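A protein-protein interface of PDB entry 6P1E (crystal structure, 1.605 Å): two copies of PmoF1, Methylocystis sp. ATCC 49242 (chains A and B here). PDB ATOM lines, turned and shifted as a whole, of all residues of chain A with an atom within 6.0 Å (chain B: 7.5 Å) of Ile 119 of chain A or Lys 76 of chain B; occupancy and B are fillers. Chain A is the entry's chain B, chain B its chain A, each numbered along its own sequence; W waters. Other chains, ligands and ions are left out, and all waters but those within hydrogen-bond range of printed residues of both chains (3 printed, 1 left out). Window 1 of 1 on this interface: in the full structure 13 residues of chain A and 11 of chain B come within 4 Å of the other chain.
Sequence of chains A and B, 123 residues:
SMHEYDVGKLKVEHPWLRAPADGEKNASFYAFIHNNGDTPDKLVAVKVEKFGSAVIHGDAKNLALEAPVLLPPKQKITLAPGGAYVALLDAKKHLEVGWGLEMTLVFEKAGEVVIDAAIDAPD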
ATOM      1  N   TRP A  16       5.011  -9.736  13.817  1.00  0.00           N
ATOM      2  CA  TRP A  16       5.979  -8.656  13.880  1.00  0.00           C
ATOM      3  C   TRP A  16       7.224  -9.007  13.092  1.00  0.00           C
ATOM      4  O   TRP A  16       7.428 -10.154  12.710  1.00  0.00           O
ATOM      5  CB  TRP A  16       6.353  -8.329  15.329  1.00  0.00           C
ATOM      6  CG  TRP A  16       7.104  -9.408  16.070  1.00  0.00           C
ATOM      7  CD1 TRP A  16       6.608 -10.596  16.523  1.00  0.00           C
ATOM      8  CD2 TRP A  16       8.480  -9.372  16.471  1.00  0.00           C
ATOM      9  NE1 TRP A  16       7.591 -11.307  17.169  1.00  0.00           N
ATOM     10  CE2 TRP A  16       8.753 -10.575  17.153  1.00  0.00           C
ATOM     11  CE3 TRP A  16       9.513  -8.442  16.313  1.00  0.00           C
ATOM     12  CZ2 TRP A  16      10.008 -10.875  17.672  1.00  0.00           C
ATOM     13  CZ3 TRP A  16      10.758  -8.740  16.831  1.00  0.00           C
ATOM     14  CH2 TRP A  16      10.995  -9.945  17.503  1.00  0.00           C
ATOM     15  N   LEU A  17       8.055  -8.009  12.841  1.00  0.00           N
ATOM     16  CA  LEU A  17       9.311  -8.267  12.164  1.00  0.00           C
ATOM     17  C   LEU A  17      10.413  -7.383  12.693  1.00  0.00           C
ATOM     18  O   LEU A  17      10.167  -6.286  13.199  1.00  0.00           O
ATOM     19  CB  LEU A  17       9.159  -8.068  10.658  1.00  0.00           C
ATOM     20  CG  LEU A  17       8.723  -6.679  10.201  1.00  0.00           C
ATOM     21  CD1 LEU A  17       9.812  -6.039   9.353  1.00  0.00           C
ATOM     22  CD2 LEU A  17       7.417  -6.772   9.430  1.00  0.00           C
ATOM     23  N   ARG A  18      11.634  -7.885  12.572  1.00  0.00           N
ATOM     24  CA  ARG A  18      12.812  -7.118  12.911  1.00  0.00           C
ATOM     25  C   ARG A  18      13.360  -6.512  11.632  1.00  0.00           C
ATOM     26  O   ARG A  18      13.743  -7.234  10.710  1.00  0.00           O
ATOM     27  CB  ARG A  18      13.856  -7.997  13.593  1.00  0.00           C
ATOM     28  CG  ARG A  18      15.075  -7.239  14.080  1.00  0.00           C
ATOM     29  CD  ARG A  18      15.644  -7.894  15.319  1.00  0.00           C
ATOM     30  NE  ARG A  18      14.795  -7.666  16.487  1.00  0.00           N
ATOM     31  CZ  ARG A  18      14.686  -8.500  17.517  1.00  0.00           C
ATOM     32  NH1 ARG A  18      15.364  -9.641  17.535  1.00  0.00           N
ATOM     33  NH2 ARG A  18      13.888  -8.197  18.532  1.00  0.00           N
ATOM     34  N   ALA A  19      13.372  -5.185  11.579  1.00  0.00           N
ATOM     35  CA  ALA A  19      13.771  -4.462  10.380  1.00  0.00           C
ATOM     36  C   ALA A  19      15.217  -4.776  10.023  1.00  0.00           C
ATOM     37  O   ALA A  19      15.989  -5.206  10.881  1.00  0.00           O
ATOM     38  CB  ALA A  19      13.584  -2.970  10.578  1.00  0.00           C
ATOM     39  N   LEU A  95      12.980   0.818   6.315  1.00  0.00           N
ATOM     40  CA  LEU A  95      11.891   0.644   7.271  1.00  0.00           C
ATOM     41  C   LEU A  95      11.966   1.580   8.476  1.00  0.00           C
ATOM     42  O   LEU A  95      13.014   1.714   9.111  1.00  0.00           O
ATOM     43  CB  LEU A  95      11.867  -0.806   7.762  1.00  0.00           C
ATOM     44  CG  LEU A  95      11.225  -1.850   6.847  1.00  0.00           C
ATOM     45  CD1 LEU A  95      11.309  -3.229   7.447  1.00  0.00           C
ATOM     46  CD2 LEU A  95       9.785  -1.512   6.620  1.00  0.00           C
ATOM     47  N   GLU A  96      10.841   2.226   8.771  1.00  0.00           N
ATOM     48  CA  GLU A  96      10.648   2.994  10.002  1.00  0.00           C
ATOM     49  C   GLU A  96       9.589   2.351  10.905  1.00  0.00           C
ATOM     50  O   GLU A  96       8.551   1.896  10.428  1.00  0.00           O
ATOM     51  CB  GLU A  96      10.302   4.450   9.699  1.00  0.00           C
ATOM     52  CG  GLU A  96      11.530   5.270   9.315  1.00  0.00           C
ATOM     53  CD  GLU A  96      11.218   6.727   9.041  1.00  0.00           C
ATOM     54  OE1 GLU A  96      10.327   7.007   8.213  1.00  0.00           O
ATOM     55  OE2 GLU A  96      11.869   7.595   9.659  1.00  0.00           O
ATOM     56  N   VAL A  97       9.873   2.309  12.203  1.00  0.00           N
ATOM     57  CA  VAL A  97       9.089   1.552  13.180  1.00  0.00           C
ATOM     58  C   VAL A  97       7.603   1.896  13.179  1.00  0.00           C
ATOM     59  O   VAL A  97       6.759   1.003  13.251  1.00  0.00           O
ATOM     60  CB  VAL A  97       9.645   1.789  14.600  1.00  0.00           C
ATOM     61  CG1 VAL A  97       8.651   1.358  15.684  1.00  0.00           C
ATOM     62  CG2 VAL A  97      10.940   1.058  14.760  1.00  0.00           C
ATOM     63  N   GLY A  98       7.286   3.185  13.114  1.00  0.00           N
ATOM     64  CA  GLY A  98       5.909   3.633  13.192  1.00  0.00           C
ATOM     65  C   GLY A  98       5.087   3.083  12.044  1.00  0.00           C
ATOM     66  O   GLY A  98       3.858   3.042  12.106  1.00  0.00           O
ATOM     67  N   TRP A  99       5.774   2.650  10.992  1.00  0.00           N
ATOM     68  CA  TRP A  99       5.107   2.111   9.825  1.00  0.00           C
ATOM     69  C   TRP A  99       4.703   0.695  10.186  1.00  0.00           C
ATOM     70  O   TRP A  99       5.287   0.093  11.085  1.00  0.00           O
ATOM     71  CB  TRP A  99       6.029   2.074   8.603  1.00  0.00           C
ATOM     72  CG  TRP A  99       6.630   3.379   8.199  1.00  0.00           C
ATOM     73  CD1 TRP A  99       6.440   4.596   8.787  1.00  0.00           C
ATOM     74  CD2 TRP A  99       7.545   3.593   7.119  1.00  0.00           C
ATOM     75  NE1 TRP A  99       7.178   5.556   8.135  1.00  0.00           N
ATOM     76  CE2 TRP A  99       7.862   4.965   7.104  1.00  0.00           C
ATOM     77  CE3 TRP A  99       8.123   2.756   6.159  1.00  0.00           C
ATOM     78  CZ2 TRP A  99       8.736   5.519   6.169  1.00  0.00           C
ATOM     79  CZ3 TRP A  99       8.986   3.309   5.228  1.00  0.00           C
ATOM     80  CH2 TRP A  99       9.284   4.677   5.241  1.00  0.00           C
ATOM     81  N   GLY A 100       3.695   0.168   9.508  1.00  0.00           N
ATOM     82  CA  GLY A 100       3.334  -1.225   9.667  1.00  0.00           C
ATOM     83  C   GLY A 100       3.738  -1.858   8.357  1.00  0.00           C
ATOM     84  O   GLY A 100       4.165  -1.149   7.445  1.00  0.00           O
ATOM     85  N   LEU A 101       3.622  -3.175   8.249  1.00  0.00           N
ATOM     86  CA  LEU A 101       3.938  -3.838   6.995  1.00  0.00           C
ATOM     87  C   LEU A 101       2.799  -4.773   6.650  1.00  0.00           C
ATOM     88  O   LEU A 101       2.528  -5.732   7.371  1.00  0.00           O
ATOM     89  CB  LEU A 101       5.259  -4.607   7.076  1.00  0.00           C
ATOM     90  CG  LEU A 101       5.660  -5.281   5.760  1.00  0.00           C
ATOM     91  CD1 LEU A 101       6.071  -4.233   4.735  1.00  0.00           C
ATOM     92  CD2 LEU A 101       6.772  -6.297   5.963  1.00  0.00           C
ATOM     93  N   ALA A 117       1.867  -6.301  10.001  1.00  0.00           N
ATOM     94  CA  ALA A 117       2.920  -6.686  10.927  1.00  0.00           C
ATOM     95  C   ALA A 117       3.549  -5.451  11.545  1.00  0.00           C
ATOM     96  O   ALA A 117       3.836  -4.472  10.860  1.00  0.00           O
ATOM     97  CB  ALA A 117       3.972  -7.524  10.221  1.00  0.00           C
ATOM     98  N   ALA A 118       3.748  -5.497  12.853  1.00  0.00           N
ATOM     99  CA  ALA A 118       4.366  -4.386  13.550  1.00  0.00           C
ATOM    100  C   ALA A 118       5.893  -4.470  13.396  1.00  0.00           C
ATOM    101  O   ALA A 118       6.449  -5.562  13.294  1.00  0.00           O
ATOM    102  CB  ALA A 118       3.937  -4.393  14.984  1.00  0.00           C
ATOM    103  N   ILE A 119       6.564  -3.321  13.360  1.00  0.00           N
ATOM    104  CA  ILE A 119       7.989  -3.287  13.027  1.00  0.00           C
ATOM    105  C   ILE A 119       8.914  -2.952  14.201  1.00  0.00           C
ATOM    106  O   ILE A 119       8.766  -1.919  14.849  1.00  0.00           O
ATOM    107  CB  ILE A 119       8.244  -2.272  11.891  1.00  0.00           C
ATOM    108  CG1 ILE A 119       7.458  -2.691  10.645  1.00  0.00           C
ATOM    109  CG2 ILE A 119       9.736  -2.168  11.569  1.00  0.00           C
ATOM    110  CD1 ILE A 119       7.484  -1.681   9.529  1.00  0.00           C
ATOM    111  N   ASP A 120       9.847  -3.865  14.468  1.00  0.00           N
ATOM    112  CA  ASP A 120      10.945  -3.660  15.417  1.00  0.00           C
ATOM    113  C   ASP A 120      12.213  -3.232  14.663  1.00  0.00           C
ATOM    114  O   ASP A 120      12.764  -4.038  13.916  1.00  0.00           O
ATOM    115  CB  ASP A 120      11.226  -4.950  16.196  1.00  0.00           C
ATOM    116  CG  ASP A 120      12.053  -4.718  17.448  1.00  0.00           C
ATOM    117  OD1 ASP A 120      11.968  -3.617  18.034  1.00  0.00           O
ATOM    118  OD2 ASP A 120      12.780  -5.649  17.856  1.00  0.00           O
ATOM    119  N   ALA A 121      12.683  -1.997  14.844  1.00  0.00           N
ATOM    120  CA  ALA A 121      13.894  -1.528  14.149  1.00  0.00           C
ATOM    121  C   ALA A 121      15.181  -1.234  14.964  1.00  0.00           C
ATOM    122  O   ALA A 121      16.261  -1.345  14.389  1.00  0.00           O
ATOM    123  CB  ALA A 121      13.550  -0.282  13.366  1.00  0.00           C
ATOM    124  N   PRO A 122      15.090  -0.846  16.262  1.00  0.00           N
ATOM    125  CA  PRO A 122      16.261  -0.355  17.020  1.00  0.00           C
ATOM    126  C   PRO A 122      17.658  -0.806  16.571  1.00  0.00           C
ATOM    127  O   PRO A 122      18.515   0.057  16.375  1.00  0.00           O
ATOM    128  CB  PRO A 122      15.992  -0.890  18.435  1.00  0.00           C
ATOM    129  CG  PRO A 122      14.535  -1.282  18.459  1.00  0.00           C
ATOM    130  CD  PRO A 122      13.925  -0.887  17.159  1.00  0.00           C
ATOM    131  N   LYS B  11       0.717  -0.996  27.550  1.00  0.00           N
ATOM    132  CA  LYS B  11       0.049  -2.207  27.101  1.00  0.00           C
ATOM    133  C   LYS B  11       1.066  -3.343  27.029  1.00  0.00           C
ATOM    134  O   LYS B  11       2.116  -3.202  26.411  1.00  0.00           O
ATOM    135  CB  LYS B  11      -0.627  -1.983  25.743  1.00  0.00           C
ATOM    136  CG  LYS B  11      -1.492  -3.149  25.291  1.00  0.00           C
ATOM    137  CD  LYS B  11      -2.231  -2.843  23.994  1.00  0.00           C
ATOM    138  CE  LYS B  11      -3.535  -2.107  24.242  1.00  0.00           C
ATOM    139  NZ  LYS B  11      -4.356  -1.989  23.007  1.00  0.00           N
ATOM    140  N   PHE B  32       5.765  -8.198  24.588  1.00  0.00           N
ATOM    141  CA  PHE B  32       5.795  -6.955  23.839  1.00  0.00           C
ATOM    142  C   PHE B  32       5.163  -5.879  24.704  1.00  0.00           C
ATOM    143  O   PHE B  32       4.012  -6.016  25.124  1.00  0.00           O
ATOM    144  CB  PHE B  32       5.062  -7.108  22.508  1.00  0.00           C
ATOM    145  CG  PHE B  32       5.493  -8.311  21.722  1.00  0.00           C
ATOM    146  CD1 PHE B  32       6.487  -8.209  20.760  1.00  0.00           C
ATOM    147  CD2 PHE B  32       4.919  -9.547  21.955  1.00  0.00           C
ATOM    148  CE1 PHE B  32       6.889  -9.314  20.040  1.00  0.00           C
ATOM    149  CE2 PHE B  32       5.321 -10.658  21.241  1.00  0.00           C
ATOM    150  CZ  PHE B  32       6.306 -10.541  20.281  1.00  0.00           C
ATOM    151  N   ILE B  33       5.925  -4.831  24.999  1.00  0.00           N
ATOM    152  CA  ILE B  33       5.450  -3.776  25.883  1.00  0.00           C
ATOM    153  C   ILE B  33       5.384  -2.443  25.154  1.00  0.00           C
ATOM    154  O   ILE B  33       6.388  -1.946  24.640  1.00  0.00           O
ATOM    155  CB  ILE B  33       6.338  -3.642  27.130  1.00  0.00           C
ATOM    156  CG1 ILE B  33       6.492  -5.003  27.816  1.00  0.00           C
ATOM    157  CG2 ILE B  33       5.740  -2.618  28.090  1.00  0.00           C
ATOM    158  CD1 ILE B  33       7.474  -5.015  28.969  1.00  0.00           C
ATOM    159  N   HIS B  34       4.183  -1.886  25.097  1.00  0.00           N
ATOM    160  CA  HIS B  34       3.948  -0.611  24.453  1.00  0.00           C
ATOM    161  C   HIS B  34       3.719   0.476  25.490  1.00  0.00           C
ATOM    162  O   HIS B  34       2.860   0.332  26.352  1.00  0.00           O
ATOM    163  CB  HIS B  34       2.741  -0.705  23.521  1.00  0.00           C
ATOM    164  CG  HIS B  34       2.928  -1.683  22.404  1.00  0.00           C
ATOM    165  ND1 HIS B  34       3.059  -1.295  21.088  1.00  0.00           N
ATOM    166  CD2 HIS B  34       2.970  -3.037  22.404  1.00  0.00           C
ATOM    167  CE1 HIS B  34       3.211  -2.365  20.329  1.00  0.00           C
ATOM    168  NE2 HIS B  34       3.156  -3.436  21.103  1.00  0.00           N
ATOM    169  N   ASN B  35       4.498   1.550  25.416  1.00  0.00           N
ATOM    170  CA  ASN B  35       4.213   2.742  26.207  1.00  0.00           C
ATOM    171  C   ASN B  35       3.573   3.783  25.301  1.00  0.00           C
ATOM    172  O   ASN B  35       4.255   4.467  24.539  1.00  0.00           O
ATOM    173  CB  ASN B  35       5.475   3.304  26.859  1.00  0.00           C
ATOM    174  CG  ASN B  35       5.176   4.464  27.800  1.00  0.00           C
ATOM    175  OD1 ASN B  35       4.051   4.967  27.850  1.00  0.00           O
ATOM    176  ND2 ASN B  35       6.183   4.897  28.544  1.00  0.00           N
ATOM    177  N   ASN B  36       2.252   3.885  25.388  1.00  0.00           N
ATOM    178  CA  ASN B  36       1.484   4.790  24.544  1.00  0.00           C
ATOM    179  C   ASN B  36       1.224   6.143  25.210  1.00  0.00           C
ATOM    180  O   ASN B  36       0.443   6.950  24.706  1.00  0.00           O
ATOM    181  CB  ASN B  36       0.171   4.113  24.153  1.00  0.00           C
ATOM    182  CG  ASN B  36       0.391   2.897  23.266  1.00  0.00           C
ATOM    183  OD1 ASN B  36       1.259   2.904  22.393  1.00  0.00           O
ATOM    184  ND2 ASN B  36      -0.372   1.837  23.507  1.00  0.00           N
ATOM    185  N   LEU B  70      13.728  -0.235  30.331  1.00  0.00           N
ATOM    186  CA  LEU B  70      13.299   1.150  30.211  1.00  0.00           C
ATOM    187  C   LEU B  70      12.213   1.248  29.157  1.00  0.00           C
ATOM    188  O   LEU B  70      12.312   0.629  28.097  1.00  0.00           O
ATOM    189  CB  LEU B  70      14.474   2.060  29.857  1.00  0.00           C
ATOM    190  CG  LEU B  70      15.685   1.985  30.791  1.00  0.00           C
ATOM    191  CD1 LEU B  70      16.722   3.028  30.397  1.00  0.00           C
ATOM    192  CD2 LEU B  70      15.274   2.160  32.244  1.00  0.00           C
ATOM    193  N   LEU B  71      11.179   2.026  29.461  1.00  0.00           N
ATOM    194  CA  LEU B  71      10.024   2.171  28.582  1.00  0.00           C
ATOM    195  C   LEU B  71       9.794   3.647  28.277  1.00  0.00           C
ATOM    196  O   LEU B  71       8.961   4.291  28.909  1.00  0.00           O
ATOM    197  CB  LEU B  71       8.779   1.557  29.225  1.00  0.00           C
ATOM    198  CG  LEU B  71       8.905   0.074  29.587  1.00  0.00           C
ATOM    199  CD1 LEU B  71       7.765  -0.345  30.495  1.00  0.00           C
ATOM    200  CD2 LEU B  71       8.946  -0.790  28.340  1.00  0.00           C
ATOM    201  N   PRO B  72      10.550   4.189  27.312  1.00  0.00           N
ATOM    202  CA  PRO B  72      10.384   5.596  26.931  1.00  0.00           C
ATOM    203  C   PRO B  72       8.991   5.875  26.370  1.00  0.00           C
ATOM    204  O   PRO B  72       8.352   4.968  25.836  1.00  0.00           O
ATOM    205  CB  PRO B  72      11.465   5.809  25.866  1.00  0.00           C
ATOM    206  CG  PRO B  72      11.826   4.451  25.390  1.00  0.00           C
ATOM    207  CD  PRO B  72      11.611   3.528  26.536  1.00  0.00           C
ATOM    208  N   PRO B  73       8.524   7.126  26.483  1.00  0.00           N
ATOM    209  CA  PRO B  73       7.183   7.470  25.998  1.00  0.00           C
ATOM    210  C   PRO B  73       7.014   7.279  24.491  1.00  0.00           C
ATOM    211  O   PRO B  73       7.955   7.498  23.725  1.00  0.00           O
ATOM    212  CB  PRO B  73       7.040   8.947  26.383  1.00  0.00           C
ATOM    213  CG  PRO B  73       8.434   9.449  26.547  1.00  0.00           C
ATOM    214  CD  PRO B  73       9.234   8.290  27.039  1.00  0.00           C
ATOM    215  N   LYS B  74       5.812   6.865  24.093  1.00  0.00           N
ATOM    216  CA  LYS B  74       5.441   6.691  22.689  1.00  0.00           C
ATOM    217  C   LYS B  74       6.373   5.733  21.962  1.00  0.00           C
ATOM    218  O   LYS B  74       6.652   5.898  20.772  1.00  0.00           O
ATOM    219  CB  LYS B  74       5.428   8.040  21.964  1.00  0.00           C
ATOM    220  CG  LYS B  74       4.493   9.061  22.578  1.00  0.00           C
ATOM    221  CD  LYS B  74       3.053   8.579  22.569  1.00  0.00           C
ATOM    222  CE  LYS B  74       2.103   9.680  23.009  1.00  0.00           C
ATOM    223  NZ  LYS B  74       0.682   9.239  22.968  1.00  0.00           N
ATOM    224  N   GLN B  75       6.839   4.718  22.679  1.00  0.00           N
ATOM    225  CA  GLN B  75       7.692   3.702  22.091  1.00  0.00           C
ATOM    226  C   GLN B  75       7.280   2.340  22.602  1.00  0.00           C
ATOM    227  O   GLN B  75       6.629   2.218  23.642  1.00  0.00           O
ATOM    228  CB  GLN B  75       9.161   3.956  22.425  1.00  0.00           C
ATOM    229  CG  GLN B  75       9.747   5.179  21.753  1.00  0.00           C
ATOM    230  CD  GLN B  75      11.261   5.210  21.827  1.00  0.00           C
ATOM    231  OE1 GLN B  75      11.931   4.215  21.548  1.00  0.00           O
ATOM    232  NE2 GLN B  75      11.806   6.345  22.238  1.00  0.00           N
ATOM    233  N   LYS B  76       7.686   1.316  21.865  1.00  0.00           N
ATOM    234  CA  LYS B  76       7.446  -0.061  22.251  1.00  0.00           C
ATOM    235  C   LYS B  76       8.774  -0.788  22.379  1.00  0.00           C
ATOM    236  O   LYS B  76       9.752  -0.441  21.704  1.00  0.00           O
ATOM    237  CB  LYS B  76       6.528  -0.739  21.234  1.00  0.00           C
ATOM    238  CG  LYS B  76       7.063  -0.716  19.824  1.00  0.00           C
ATOM    239  CD  LYS B  76       5.942  -0.612  18.793  1.00  0.00           C
ATOM    240  CE  LYS B  76       6.497  -0.357  17.400  1.00  0.00           C
ATOM    241  NZ  LYS B  76       5.588  -0.704  16.292  1.00  0.00           N
ATOM    242  N   ILE B  77       8.798  -1.785  23.257  1.00  0.00           N
ATOM    243  CA  ILE B  77       9.983  -2.592  23.500  1.00  0.00           C
ATOM    244  C   ILE B  77       9.627  -4.060  23.340  1.00  0.00           C
ATOM    245  O   ILE B  77       8.596  -4.520  23.841  1.00  0.00           O
ATOM    246  CB  ILE B  77      10.561  -2.349  24.913  1.00  0.00           C
ATOM    247  CG1 ILE B  77      10.859  -0.861  25.128  1.00  0.00           C
ATOM    248  CG2 ILE B  77      11.813  -3.195  25.141  1.00  0.00           C
ATOM    249  CD1 ILE B  77      11.939  -0.293  24.221  1.00  0.00           C
ATOM    250  N   THR B  78      10.476  -4.783  22.622  1.00  0.00           N
ATOM    251  CA  THR B  78      10.326  -6.221  22.467  1.00  0.00           C
ATOM    252  C   THR B  78      11.285  -6.954  23.374  1.00  0.00           C
ATOM    253  O   THR B  78      12.497  -6.748  23.296  1.00  0.00           O
ATOM    254  CB  THR B  78      10.613  -6.682  21.035  1.00  0.00           C
ATOM    255  OG1 THR B  78       9.943  -5.829  20.114  1.00  0.00           O
ATOM    256  CG2 THR B  78      10.172  -8.129  20.836  1.00  0.00           C
HETATM  257  O   HOH W   1      14.396  -8.339  21.864  1.00  0.00           O
HETATM  258  O   HOH W   2      10.056  -2.723  19.241  1.00  0.00           O
HETATM  259  O   HOH W   3      12.715  -3.640  21.188  1.00  0.00           O
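Of the 15 printed residues of chain B, 3 touch a printed residue of chain A.
Hydrophobic or aromatic side chains of chain B that line the printed part of chain A: Phe 32.
Printed residues of chain A that touch a printed residue of chain B: Trp 16, Val 97, Ile 119 and Asp 120.
Among the printed residues, merely in contact across the chains: Val 97 of chain A with Lys 76 of chain B, Trp 16 of chain A with Phe 32 of chain B, Asp 120 of chain A with Thr 78 of chain B, Ile 119 of chain A with Lys 76 of chain B and Trp 16 of chain A with Thr 78 of chain B.
Water W2 lies within hydrogen-bond range of OD1 of Asp 120 of chain A (2.4 Å), OG1 of Thr 78 of chain B (3.2 Å) and O of Lys 76 of chain B (3.4 Å).
Water W1 lies within hydrogen-bond range of the backbone carbonyl oxygen of Thr 78 of chain B (2.9 Å) and the guanidinium group of Arg 18 of chain A (3.4 Å).
Water W3 lies within hydrogen-bond range of N of Thr 78 of chain B (2.9 Å) and OD1 of Asp 120 of chain A (3.2 Å).
The backbone NH (N) of Asp 120 of chain A sits at hydrogen-bond distance from the backbone carbonyl oxygen (O) of Leu 17 of chain A, 2.8 Å away.
NH2 of Arg 18 of chain A is in salt-bridge range of OD2 of Asp 120 of chain A (2.9 Å).
The backbone NH (N) of Ala 19 of chain A is in hydrogen-bond range of the backbone carbonyl oxygen (O) of Asp 120 of chain A (2.7 Å).
No position is printed for both chains.
Of the 5 pairs that touch across the chains among the printed residues, none has its exchanged pair printed and touching as well.
Of chain B, only Lys 76 (3.7 Å) comes within 4 Å of Ile 119 of chain A.
Lys 76 of chain B touches just these residues of chain A: Val 97 (3.2 Å) and Ile 119 (3.7 Å).
Of the printed residues of chain B, Asp 120 of chain A touches Thr 78.
Printed residues of chain B within 4 Å of Trp 16 of chain A: Phe 32 (3.5 Å) and Thr 78 (3.9 Å).
Printed residues of chain A within 4 Å of Phe 32 of chain B: Trp 16 (3.5 Å).
Of the printed residues of chain B, Val 97 of chain A touches Lys 76.
The nearest residue of chain B that does not touch Ile 119 of chain A is Thr 78 of chain B (6.7 Å).
The nearest printed residue of chain A that does not touch Thr 78 of chain B is Arg 18 of chain A (4.4 Å).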
